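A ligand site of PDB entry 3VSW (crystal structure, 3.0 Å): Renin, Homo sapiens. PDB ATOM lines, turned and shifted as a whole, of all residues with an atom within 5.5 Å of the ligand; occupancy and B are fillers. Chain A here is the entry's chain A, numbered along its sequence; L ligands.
N3 of the ligand lies within salt-bridge range of OD2 of Asp 226, 2.8 Å away. The backbone carbonyl oxygen of Gly 228 sits at hydrogen-bond distance from a nitrogen (N3) of the ligand (3.0 Å). An oxygen (O3) of the ligand is in hydrogen-bond range of the backbone NH of Ser 41. An oxygen (O4) of the ligand lies within hydrogen-bond range of the backbone NH of Ser 84 (3.3 Å). The side-chain amide oxygen (OE1) of Gln 135 lies close to an oxygen (O5) of the ligand (3.4 Å). N4 of the ligand lies within hydrogen-bond range of O of Gly 40 (3.1 Å). The side-chain hydroxyl (OG1) of Thr 85 sits at hydrogen-bond distance from an oxygen (O6) of the ligand (2.7 Å). OD1 of Asp 38 is in salt-bridge range of N3 of the ligand, 2.9 Å away.
The backbone NH of Ala 317 is in hydrogen-bond range of the backbone carbonyl oxygen of Ala 229, 2.8 Å away. The side-chain carboxylate (OD1) of Asp 226 lies within hydrogen-bond range of the backbone NH (N) of Gly 228 (2.9 Å). OD2 of Asp 38 is in hydrogen-bond range of OG of Ser 41 (2.6 Å). OD1 of Asp 38 sits at hydrogen-bond distance from N of Gly 40. O of Thr 227 is in hydrogen-bond range of OH of Tyr 162 (2.8 Å). The backbone NH (N) of Thr 227 is in hydrogen-bond range of the side-chain hydroxyl (OG1) of Thr 39, at 2.7 Å. N of Ala 317 sits close to O of Ser 230. O of Leu 121 is in hydrogen-bond range of NE2 of Gln 19, at 2.9 Å.
Merely in contact with the ligand: Thr 18 (3.1 Å), Thr 227 (3.2 Å), Arg 82 (3.4 Å), Tyr 20 (3.5 Å), Ile 137 (3.5 Å), Ser 230 (3.5 Å), Tyr 83 (3.6 Å), Tyr 162 (3.6 Å), Phe 124 (3.6 Å), Ile 305 (3.6 Å), Leu 224 (3.7 Å), Ala 122 (3.7 Å), Pro 118 (3.7 Å), Phe 119 (3.8 Å), Ala 229 (3.8 Å) and Gln 19 (3.99 Å). Hydrophobic or aromatic side chains within 4 Å of the ligand: Tyr 20, Tyr 83, Pro 118, Phe 119, Ala 122, Phe 124, Ile 137, Tyr 162, Leu 224 and Ile 305. Within 4 Å of the ligand: Thr 18, Gln 19, Tyr 20, Asp 38, Gly 40, Ser 41, Arg 82, Tyr 83, Ser 84, Thr 85, Pro 118, Phe 119, Ala 122, Phe 124, Gln 135, Ile 137, Tyr 162, Leu 224, Asp 226, Thr 227, Gly 228, Ala 229, Ser 230 and Ile 305. The nearest printed residue that does not touch the ligand is Val 127 (4.02 Å).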
ATOM      1  N   THR A  18      33.904  -2.414  -4.683  1.00  0.00           N
ATOM      2  CA  THR A  18      33.605  -3.219  -3.527  1.00  0.00           C
ATOM      3  C   THR A  18      32.249  -2.879  -2.919  1.00  0.00           C
ATOM      4  O   THR A  18      31.739  -3.617  -2.080  1.00  0.00           O
ATOM      5  CB  THR A  18      34.642  -2.981  -2.471  1.00  0.00           C
ATOM      6  OG1 THR A  18      34.540  -1.623  -2.041  1.00  0.00           O
ATOM      7  CG2 THR A  18      36.034  -3.210  -3.034  1.00  0.00           C
ATOM      8  N   GLN A  19      31.684  -1.752  -3.312  1.00  0.00           N
ATOM      9  CA  GLN A  19      30.390  -1.337  -2.776  1.00  0.00           C
ATOM     10  C   GLN A  19      29.551  -0.680  -3.843  1.00  0.00           C
ATOM     11  O   GLN A  19      29.963   0.326  -4.407  1.00  0.00           O
ATOM     12  CB  GLN A  19      30.601  -0.339  -1.637  1.00  0.00           C
ATOM     13  CG  GLN A  19      31.112  -0.951  -0.365  1.00  0.00           C
ATOM     14  CD  GLN A  19      31.209   0.065   0.739  1.00  0.00           C
ATOM     15  OE1 GLN A  19      30.300   0.877   0.923  1.00  0.00           O
ATOM     16  NE2 GLN A  19      32.311   0.033   1.482  1.00  0.00           N
ATOM     17  N   TYR A  20      28.365  -1.238  -4.089  1.00  0.00           N
ATOM     18  CA  TYR A  20      27.438  -0.693  -5.077  1.00  0.00           C
ATOM     19  C   TYR A  20      26.116  -0.390  -4.398  1.00  0.00           C
ATOM     20  O   TYR A  20      25.452  -1.300  -3.905  1.00  0.00           O
ATOM     21  CB  TYR A  20      27.190  -1.703  -6.189  1.00  0.00           C
ATOM     22  CG  TYR A  20      28.388  -1.982  -7.082  1.00  0.00           C
ATOM     23  CD1 TYR A  20      29.435  -2.802  -6.664  1.00  0.00           C
ATOM     24  CD2 TYR A  20      28.444  -1.423  -8.354  1.00  0.00           C
ATOM     25  CE1 TYR A  20      30.517  -3.056  -7.515  1.00  0.00           C
ATOM     26  CE2 TYR A  20      29.516  -1.657  -9.194  1.00  0.00           C
ATOM     27  CZ  TYR A  20      30.543  -2.474  -8.780  1.00  0.00           C
ATOM     28  OH  TYR A  20      31.605  -2.663  -9.647  1.00  0.00           O
ATOM     29  N   VAL A  36      22.112  -0.893  -0.125  1.00  0.00           N
ATOM     30  CA  VAL A  36      22.670  -1.933  -0.958  1.00  0.00           C
ATOM     31  C   VAL A  36      21.512  -2.852  -1.317  1.00  0.00           C
ATOM     32  O   VAL A  36      20.708  -3.192  -0.463  1.00  0.00           O
ATOM     33  CB  VAL A  36      23.716  -2.756  -0.191  1.00  0.00           C
ATOM     34  CG1 VAL A  36      23.950  -4.084  -0.892  1.00  0.00           C
ATOM     35  CG2 VAL A  36      25.016  -1.980  -0.094  1.00  0.00           C
ATOM     36  N   ASP A  38      20.611  -6.254  -1.934  1.00  0.00           N
ATOM     37  CA  ASP A  38      21.143  -7.563  -1.590  1.00  0.00           C
ATOM     38  C   ASP A  38      20.277  -8.797  -1.838  1.00  0.00           C
ATOM     39  O   ASP A  38      19.335  -9.076  -1.093  1.00  0.00           O
ATOM     40  CB  ASP A  38      21.573  -7.506  -0.112  1.00  0.00           C
ATOM     41  CG  ASP A  38      21.954  -8.842   0.440  1.00  0.00           C
ATOM     42  OD1 ASP A  38      22.625  -9.593  -0.270  1.00  0.00           O
ATOM     43  OD2 ASP A  38      21.602  -9.130   1.603  1.00  0.00           O
ATOM     44  N   THR A  39      20.627  -9.559  -2.879  1.00  0.00           N
ATOM     45  CA  THR A  39      19.903 -10.774  -3.227  1.00  0.00           C
ATOM     46  C   THR A  39      20.246 -11.893  -2.259  1.00  0.00           C
ATOM     47  O   THR A  39      19.759 -13.011  -2.382  1.00  0.00           O
ATOM     48  CB  THR A  39      20.257 -11.291  -4.642  1.00  0.00           C
ATOM     49  OG1 THR A  39      21.683 -11.256  -4.821  1.00  0.00           O
ATOM     50  CG2 THR A  39      19.570 -10.468  -5.707  1.00  0.00           C
ATOM     51  N   GLY A  40      21.112 -11.588  -1.296  1.00  0.00           N
ATOM     52  CA  GLY A  40      21.509 -12.592  -0.331  1.00  0.00           C
ATOM     53  C   GLY A  40      20.594 -12.655   0.872  1.00  0.00           C
ATOM     54  O   GLY A  40      20.681 -13.591   1.671  1.00  0.00           O
ATOM     55  N   SER A  41      19.715 -11.655   1.008  1.00  0.00           N
ATOM     56  CA  SER A  41      18.788 -11.580   2.141  1.00  0.00           C
ATOM     57  C   SER A  41      17.442 -11.059   1.657  1.00  0.00           C
ATOM     58  O   SER A  41      17.309 -10.711   0.498  1.00  0.00           O
ATOM     59  CB  SER A  41      19.358 -10.656   3.223  1.00  0.00           C
ATOM     60  OG  SER A  41      19.334  -9.314   2.800  1.00  0.00           O
ATOM     61  N   SER A  42      16.445 -10.991   2.542  1.00  0.00           N
ATOM     62  CA  SER A  42      15.129 -10.525   2.139  1.00  0.00           C
ATOM     63  C   SER A  42      14.494  -9.450   3.025  1.00  0.00           C
ATOM     64  O   SER A  42      13.275  -9.225   2.958  1.00  0.00           O
ATOM     65  CB  SER A  42      14.185 -11.707   2.016  1.00  0.00           C
ATOM     66  OG  SER A  42      14.817 -12.764   1.328  1.00  0.00           O
ATOM     67  N   LEU A  81      19.065  -9.362  12.375  1.00  0.00           N
ATOM     68  CA  LEU A  81      19.512  -9.911  11.105  1.00  0.00           C
ATOM     69  C   LEU A  81      20.964 -10.344  11.224  1.00  0.00           C
ATOM     70  O   LEU A  81      21.850  -9.543  11.540  1.00  0.00           O
ATOM     71  CB  LEU A  81      19.368  -8.859  10.012  1.00  0.00           C
ATOM     72  CG  LEU A  81      17.981  -8.203  10.025  1.00  0.00           C
ATOM     73  CD1 LEU A  81      17.985  -6.957   9.148  1.00  0.00           C
ATOM     74  CD2 LEU A  81      16.939  -9.235   9.570  1.00  0.00           C
ATOM     75  N   ARG A  82      21.181 -11.640  10.991  1.00  0.00           N
ATOM     76  CA  ARG A  82      22.519 -12.199  11.091  1.00  0.00           C
ATOM     77  C   ARG A  82      23.072 -12.571   9.740  1.00  0.00           C
ATOM     78  O   ARG A  82      22.649 -13.534   9.127  1.00  0.00           O
ATOM     79  CB  ARG A  82      22.508 -13.429  12.014  1.00  0.00           C
ATOM     80  CG  ARG A  82      22.019 -13.121  13.421  1.00  0.00           C
ATOM     81  CD  ARG A  82      22.078 -14.327  14.373  1.00  0.00           C
ATOM     82  NE  ARG A  82      21.167 -14.162  15.526  1.00  0.00           N
ATOM     83  CZ  ARG A  82      19.832 -14.224  15.463  1.00  0.00           C
ATOM     84  NH1 ARG A  82      19.225 -14.453  14.298  1.00  0.00           N
ATOM     85  NH2 ARG A  82      19.106 -14.049  16.560  1.00  0.00           N
ATOM     86  N   TYR A  83      24.013 -11.770   9.284  1.00  0.00           N
ATOM     87  CA  TYR A  83      24.664 -11.985   8.004  1.00  0.00           C
ATOM     88  C   TYR A  83      25.985 -12.724   8.253  1.00  0.00           C
ATOM     89  O   TYR A  83      26.530 -12.694   9.352  1.00  0.00           O
ATOM     90  CB  TYR A  83      24.976 -10.658   7.347  1.00  0.00           C
ATOM     91  CG  TYR A  83      23.786  -9.777   7.088  1.00  0.00           C
ATOM     92  CD1 TYR A  83      23.858  -8.413   7.348  1.00  0.00           C
ATOM     93  CD2 TYR A  83      22.637 -10.270   6.494  1.00  0.00           C
ATOM     94  CE1 TYR A  83      22.821  -7.563   7.007  1.00  0.00           C
ATOM     95  CE2 TYR A  83      21.592  -9.424   6.143  1.00  0.00           C
ATOM     96  CZ  TYR A  83      21.694  -8.068   6.400  1.00  0.00           C
ATOM     97  OH  TYR A  83      20.698  -7.208   6.011  1.00  0.00           O
ATOM     98  N   SER A  84      26.499 -13.384   7.229  1.00  0.00           N
ATOM     99  CA  SER A  84      27.741 -14.120   7.351  1.00  0.00           C
ATOM    100  C   SER A  84      28.888 -13.241   7.801  1.00  0.00           C
ATOM    101  O   SER A  84      29.883 -13.720   8.328  1.00  0.00           O
ATOM    102  CB  SER A  84      28.088 -14.778   5.993  1.00  0.00           C
ATOM    103  OG  SER A  84      28.070 -13.830   4.929  1.00  0.00           O
ATOM    104  N   THR A  85      28.747 -11.928   7.614  1.00  0.00           N
ATOM    105  CA  THR A  85      29.815 -11.008   7.962  1.00  0.00           C
ATOM    106  C   THR A  85      29.492  -9.974   9.022  1.00  0.00           C
ATOM    107  O   THR A  85      30.352  -9.154   9.382  1.00  0.00           O
ATOM    108  CB  THR A  85      30.276 -10.250   6.723  1.00  0.00           C
ATOM    109  OG1 THR A  85      29.180  -9.510   6.184  1.00  0.00           O
ATOM    110  CG2 THR A  85      30.756 -11.212   5.685  1.00  0.00           C
ATOM    111  N   PRO A 118      30.802  -4.650  10.273  1.00  0.00           N
ATOM    112  CA  PRO A 118      31.446  -4.000   9.140  1.00  0.00           C
ATOM    113  C   PRO A 118      30.959  -2.598   8.770  1.00  0.00           C
ATOM    114  O   PRO A 118      31.696  -1.795   8.197  1.00  0.00           O
ATOM    115  CB  PRO A 118      31.175  -4.968   8.012  1.00  0.00           C
ATOM    116  CG  PRO A 118      29.714  -5.306   8.305  1.00  0.00           C
ATOM    117  CD  PRO A 118      29.664  -5.467   9.811  1.00  0.00           C
ATOM    118  N   PHE A 119      29.709  -2.311   9.094  1.00  0.00           N
ATOM    119  CA  PHE A 119      29.035  -1.060   8.758  1.00  0.00           C
ATOM    120  C   PHE A 119      29.759   0.266   8.948  1.00  0.00           C
ATOM    121  O   PHE A 119      29.363   1.274   8.388  1.00  0.00           O
ATOM    122  CB  PHE A 119      27.691  -1.050   9.488  1.00  0.00           C
ATOM    123  CG  PHE A 119      26.930  -2.311   9.315  1.00  0.00           C
ATOM    124  CD1 PHE A 119      26.445  -2.672   8.065  1.00  0.00           C
ATOM    125  CD2 PHE A 119      26.812  -3.211  10.372  1.00  0.00           C
ATOM    126  CE1 PHE A 119      25.857  -3.907   7.860  1.00  0.00           C
ATOM    127  CE2 PHE A 119      26.212  -4.453  10.169  1.00  0.00           C
ATOM    128  CZ  PHE A 119      25.741  -4.803   8.903  1.00  0.00           C
ATOM    129  N   LEU A 121      32.463   0.631   7.891  1.00  0.00           N
ATOM    130  CA  LEU A 121      33.218   0.658   6.645  1.00  0.00           C
ATOM    131  C   LEU A 121      32.264   0.779   5.471  1.00  0.00           C
ATOM    132  O   LEU A 121      32.672   0.767   4.314  1.00  0.00           O
ATOM    133  CB  LEU A 121      34.050  -0.617   6.478  1.00  0.00           C
ATOM    134  CG  LEU A 121      35.510  -0.687   6.957  1.00  0.00           C
ATOM    135  CD1 LEU A 121      35.583  -0.584   8.463  1.00  0.00           C
ATOM    136  CD2 LEU A 121      36.121  -1.994   6.460  1.00  0.00           C
ATOM    137  N   ALA A 122      30.978   0.917   5.785  1.00  0.00           N
ATOM    138  CA  ALA A 122      29.944   1.028   4.771  1.00  0.00           C
ATOM    139  C   ALA A 122      29.790   2.459   4.270  1.00  0.00           C
ATOM    140  O   ALA A 122      29.616   3.377   5.053  1.00  0.00           O
ATOM    141  CB  ALA A 122      28.624   0.535   5.320  1.00  0.00           C
ATOM    142  N   PHE A 124      27.395   3.241   2.554  1.00  0.00           N
ATOM    143  CA  PHE A 124      25.938   3.352   2.482  1.00  0.00           C
ATOM    144  C   PHE A 124      25.333   3.258   3.876  1.00  0.00           C
ATOM    145  O   PHE A 124      26.044   3.014   4.840  1.00  0.00           O
ATOM    146  CB  PHE A 124      25.366   2.225   1.622  1.00  0.00           C
ATOM    147  CG  PHE A 124      25.889   0.873   1.990  1.00  0.00           C
ATOM    148  CD1 PHE A 124      27.181   0.497   1.606  1.00  0.00           C
ATOM    149  CD2 PHE A 124      25.122  -0.014   2.736  1.00  0.00           C
ATOM    150  CE1 PHE A 124      27.688  -0.737   1.972  1.00  0.00           C
ATOM    151  CE2 PHE A 124      25.627  -1.255   3.107  1.00  0.00           C
ATOM    152  CZ  PHE A 124      26.910  -1.617   2.725  1.00  0.00           C
ATOM    153  N   VAL A 127      20.352  -1.728   3.899  1.00  0.00           N
ATOM    154  CA  VAL A 127      20.195  -2.862   2.997  1.00  0.00           C
ATOM    155  C   VAL A 127      18.752  -3.094   2.567  1.00  0.00           C
ATOM    156  O   VAL A 127      17.817  -2.912   3.347  1.00  0.00           O
ATOM    157  CB  VAL A 127      20.713  -4.165   3.660  1.00  0.00           C
ATOM    158  CG1 VAL A 127      20.564  -5.340   2.689  1.00  0.00           C
ATOM    159  CG2 VAL A 127      22.159  -3.987   4.098  1.00  0.00           C
ATOM    160  N   GLN A 135      13.206 -16.463   3.201  1.00  0.00           N
ATOM    161  CA  GLN A 135      14.418 -16.100   3.924  1.00  0.00           C
ATOM    162  C   GLN A 135      14.237 -14.832   4.746  1.00  0.00           C
ATOM    163  O   GLN A 135      15.084 -14.477   5.562  1.00  0.00           O
ATOM    164  CB  GLN A 135      15.582 -15.945   2.938  1.00  0.00           C
ATOM    165  CG  GLN A 135      15.851 -17.219   2.140  1.00  0.00           C
ATOM    166  CD  GLN A 135      16.178 -18.397   3.036  1.00  0.00           C
ATOM    167  OE1 GLN A 135      17.214 -18.411   3.703  1.00  0.00           O
ATOM    168  NE2 GLN A 135      15.291 -19.391   3.064  1.00  0.00           N
ATOM    169  N   ALA A 136      13.123 -14.145   4.504  1.00  0.00           N
ATOM    170  CA  ALA A 136      12.826 -12.908   5.205  1.00  0.00           C
ATOM    171  C   ALA A 136      12.706 -13.208   6.667  1.00  0.00           C
ATOM    172  O   ALA A 136      11.904 -14.046   7.068  1.00  0.00           O
ATOM    173  CB  ALA A 136      11.534 -12.324   4.689  1.00  0.00           C
ATOM    174  N   ILE A 137      13.498 -12.534   7.489  1.00  0.00           N
ATOM    175  CA  ILE A 137      13.423 -12.774   8.910  1.00  0.00           C
ATOM    176  C   ILE A 137      12.193 -12.064   9.456  1.00  0.00           C
ATOM    177  O   ILE A 137      11.899 -10.939   9.082  1.00  0.00           O
ATOM    178  CB  ILE A 137      14.710 -12.316   9.621  1.00  0.00           C
ATOM    179  CG1 ILE A 137      15.875 -13.224   9.196  1.00  0.00           C
ATOM    180  CG2 ILE A 137      14.529 -12.366  11.130  1.00  0.00           C
ATOM    181  CD1 ILE A 137      17.148 -12.954   9.921  1.00  0.00           C
ATOM    182  N   TYR A 162      26.731  -4.186 -12.627  1.00  0.00           N
ATOM    183  CA  TYR A 162      27.777  -3.573 -11.836  1.00  0.00           C
ATOM    184  C   TYR A 162      28.855  -3.173 -12.811  1.00  0.00           C
ATOM    185  O   TYR A 162      29.376  -4.019 -13.540  1.00  0.00           O
ATOM    186  CB  TYR A 162      28.349  -4.537 -10.794  1.00  0.00           C
ATOM    187  CG  TYR A 162      27.451  -4.705  -9.585  1.00  0.00           C
ATOM    188  CD1 TYR A 162      26.400  -3.816  -9.358  1.00  0.00           C
ATOM    189  CD2 TYR A 162      27.659  -5.728  -8.665  1.00  0.00           C
ATOM    190  CE1 TYR A 162      25.586  -3.940  -8.247  1.00  0.00           C
ATOM    191  CE2 TYR A 162      26.841  -5.851  -7.532  1.00  0.00           C
ATOM    192  CZ  TYR A 162      25.808  -4.947  -7.334  1.00  0.00           C
ATOM    193  OH  TYR A 162      24.970  -5.043  -6.243  1.00  0.00           O
ATOM    194  N   LEU A 224      25.780 -19.286  -4.616  1.00  0.00           N
ATOM    195  CA  LEU A 224      24.723 -18.349  -4.265  1.00  0.00           C
ATOM    196  C   LEU A 224      25.076 -17.001  -4.907  1.00  0.00           C
ATOM    197  O   LEU A 224      26.098 -16.400  -4.564  1.00  0.00           O
ATOM    198  CB  LEU A 224      24.623 -18.229  -2.754  1.00  0.00           C
ATOM    199  CG  LEU A 224      23.386 -17.515  -2.224  1.00  0.00           C
ATOM    200  CD1 LEU A 224      23.114 -17.955  -0.800  1.00  0.00           C
ATOM    201  CD2 LEU A 224      23.575 -16.013  -2.299  1.00  0.00           C
ATOM    202  N   ASP A 226      25.055 -13.682  -4.796  1.00  0.00           N
ATOM    203  CA  ASP A 226      24.874 -12.606  -3.815  1.00  0.00           C
ATOM    204  C   ASP A 226      25.254 -11.215  -4.351  1.00  0.00           C
ATOM    205  O   ASP A 226      26.437 -10.863  -4.391  1.00  0.00           O
ATOM    206  CB  ASP A 226      25.710 -12.930  -2.571  1.00  0.00           C
ATOM    207  CG  ASP A 226      25.430 -12.005  -1.419  1.00  0.00           C
ATOM    208  OD1 ASP A 226      24.663 -11.037  -1.590  1.00  0.00           O
ATOM    209  OD2 ASP A 226      25.987 -12.238  -0.328  1.00  0.00           O
ATOM    210  N   THR A 227      24.270 -10.410  -4.729  1.00  0.00           N
ATOM    211  CA  THR A 227      24.560  -9.080  -5.262  1.00  0.00           C
ATOM    212  C   THR A 227      25.068  -8.148  -4.169  1.00  0.00           C
ATOM    213  O   THR A 227      25.680  -7.114  -4.460  1.00  0.00           O
ATOM    214  CB  THR A 227      23.309  -8.425  -5.907  1.00  0.00           C
ATOM    215  OG1 THR A 227      22.248  -8.359  -4.946  1.00  0.00           O
ATOM    216  CG2 THR A 227      22.836  -9.227  -7.108  1.00  0.00           C
ATOM    217  N   GLY A 228      24.825  -8.518  -2.922  1.00  0.00           N
ATOM    218  CA  GLY A 228      25.260  -7.710  -1.788  1.00  0.00           C
ATOM    219  C   GLY A 228      26.593  -8.177  -1.254  1.00  0.00           C
ATOM    220  O   GLY A 228      26.932  -7.911  -0.105  1.00  0.00           O
ATOM    221  N   ALA A 229      27.359  -8.865  -2.107  1.00  0.00           N
ATOM    222  CA  ALA A 229      28.680  -9.375  -1.759  1.00  0.00           C
ATOM    223  C   ALA A 229      29.689  -8.716  -2.695  1.00  0.00           C
ATOM    224  O   ALA A 229      29.400  -8.507  -3.871  1.00  0.00           O
ATOM    225  CB  ALA A 229      28.711 -10.871  -1.942  1.00  0.00           C
ATOM    226  N   SER A 230      30.872  -8.390  -2.175  1.00  0.00           N
ATOM    227  CA  SER A 230      31.898  -7.751  -2.992  1.00  0.00           C
ATOM    228  C   SER A 230      32.670  -8.746  -3.851  1.00  0.00           C
ATOM    229  O   SER A 230      32.823  -8.566  -5.055  1.00  0.00           O
ATOM    230  CB  SER A 230      32.907  -6.994  -2.126  1.00  0.00           C
ATOM    231  OG  SER A 230      32.359  -5.836  -1.558  1.00  0.00           O
ATOM    232  N   ILE A 305      29.546 -20.205   4.977  1.00  0.00           N
ATOM    233  CA  ILE A 305      28.183 -19.855   5.287  1.00  0.00           C
ATOM    234  C   ILE A 305      27.468 -21.013   5.964  1.00  0.00           C
ATOM    235  O   ILE A 305      27.500 -22.156   5.494  1.00  0.00           O
ATOM    236  CB  ILE A 305      27.470 -19.417   4.001  1.00  0.00           C
ATOM    237  CG1 ILE A 305      28.184 -18.187   3.433  1.00  0.00           C
ATOM    238  CG2 ILE A 305      26.001 -19.141   4.284  1.00  0.00           C
ATOM    239  CD1 ILE A 305      27.920 -17.930   1.976  1.00  0.00           C
ATOM    240  N   THR A 309      21.798 -23.082   4.411  1.00  0.00           N
ATOM    241  CA  THR A 309      22.192 -22.520   3.128  1.00  0.00           C
ATOM    242  C   THR A 309      23.599 -22.951   2.753  1.00  0.00           C
ATOM    243  O   THR A 309      23.859 -23.332   1.609  1.00  0.00           O
ATOM    244  CB  THR A 309      22.095 -20.997   3.126  1.00  0.00           C
ATOM    245  OG1 THR A 309      20.741 -20.609   3.403  1.00  0.00           O
ATOM    246  CG2 THR A 309      22.491 -20.439   1.774  1.00  0.00           C
ATOM    247  N   ALA A 314      29.750 -18.044  -3.011  1.00  0.00           N
ATOM    248  CA  ALA A 314      28.851 -16.912  -3.188  1.00  0.00           C
ATOM    249  C   ALA A 314      29.492 -16.070  -4.293  1.00  0.00           C
ATOM    250  O   ALA A 314      30.623 -15.614  -4.145  1.00  0.00           O
ATOM    251  CB  ALA A 314      28.754 -16.121  -1.892  1.00  0.00           C
ATOM    252  N   ALA A 317      30.087  -9.260  -6.519  1.00  0.00           N
ATOM    253  CA  ALA A 317      30.499  -8.226  -7.471  1.00  0.00           C
ATOM    254  C   ALA A 317      31.620  -8.651  -8.426  1.00  0.00           C
ATOM    255  O   ALA A 317      31.537  -8.382  -9.626  1.00  0.00           O
ATOM    256  CB  ALA A 317      30.883  -6.959  -6.725  1.00  0.00           C
HETATM  257  C1  LIG L   1      26.589  -7.996   4.265  1.00  0.00           C
HETATM  258  N1  LIG L   1      25.529  -7.739   3.314  1.00  0.00           N
HETATM  259  C2  LIG L   1      25.208  -6.372   3.029  1.00  0.00           C
HETATM  260  C3  LIG L   1      26.450  -5.557   2.609  1.00  0.00           C
HETATM  261  N2  LIG L   1      27.578  -5.746   3.563  1.00  0.00           N
HETATM  262  C4  LIG L   1      27.745  -6.975   4.180  1.00  0.00           C
HETATM  263  C5  LIG L   1      28.453  -4.716   3.803  1.00  0.00           C
HETATM  264  C6  LIG L   1      29.438  -4.394   2.840  1.00  0.00           C
HETATM  265  C7  LIG L   1      30.380  -3.363   3.109  1.00  0.00           C
HETATM  266  C8  LIG L   1      30.412  -2.768   4.416  1.00  0.00           C
HETATM  267  C9  LIG L   1      29.402  -3.074   5.356  1.00  0.00           C
HETATM  268  C10 LIG L   1      28.385  -3.991   5.012  1.00  0.00           C
HETATM  269  O1  LIG L   1      29.517  -5.051   1.673  1.00  0.00           O
HETATM  270  C11 LIG L   1      29.490  -4.537   0.371  1.00  0.00           C
HETATM  271  C12 LIG L   1      28.848  -5.542  -0.590  1.00  0.00           C
HETATM  272  C13 LIG L   1      28.989  -5.004  -2.015  1.00  0.00           C
HETATM  273  O2  LIG L   1      27.796  -4.350  -2.409  1.00  0.00           O
HETATM  274  C14 LIG L   1      27.547  -4.613  -3.771  1.00  0.00           C
HETATM  275  C15 LIG L   1      24.545  -8.746   3.072  1.00  0.00           C
HETATM  276  C16 LIG L   1      25.090 -10.104   2.562  1.00  0.00           C
HETATM  277  C17 LIG L   1      24.163 -11.278   2.982  1.00  0.00           C
HETATM  278  N3  LIG L   1      25.174 -10.030   1.099  1.00  0.00           N
HETATM  279  C18 LIG L   1      24.780 -12.692   2.838  1.00  0.00           C
HETATM  280  O3  LIG L   1      22.967 -11.231   2.208  1.00  0.00           O
HETATM  281  C19 LIG L   1      23.927 -13.994   2.933  1.00  0.00           C
HETATM  282  C20 LIG L   1      23.273 -14.081   4.319  1.00  0.00           C
HETATM  283  N4  LIG L   1      21.962 -13.905   4.504  1.00  0.00           N
HETATM  284  O4  LIG L   1      23.990 -14.306   5.319  1.00  0.00           O
HETATM  285  C21 LIG L   1      24.707 -15.305   2.514  1.00  0.00           C
HETATM  286  C22 LIG L   1      21.357 -13.543   5.795  1.00  0.00           C
HETATM  287  C23 LIG L   1      20.409 -14.569   6.429  1.00  0.00           C
HETATM  288  C24 LIG L   1      19.498 -15.093   5.286  1.00  0.00           C
HETATM  289  N5  LIG L   1      18.579 -14.245   4.739  1.00  0.00           N
HETATM  290  C25 LIG L   1      21.203 -15.755   7.055  1.00  0.00           C
HETATM  291  C26 LIG L   1      19.481 -13.901   7.496  1.00  0.00           C
HETATM  292  O5  LIG L   1      19.622 -16.241   4.864  1.00  0.00           O
HETATM  293  C27 LIG L   1      23.823 -16.614   2.541  1.00  0.00           C
HETATM  294  C28 LIG L   1      25.543 -15.276   1.218  1.00  0.00           C
HETATM  295  O6  LIG L   1      28.788  -7.298   4.714  1.00  0.00           O
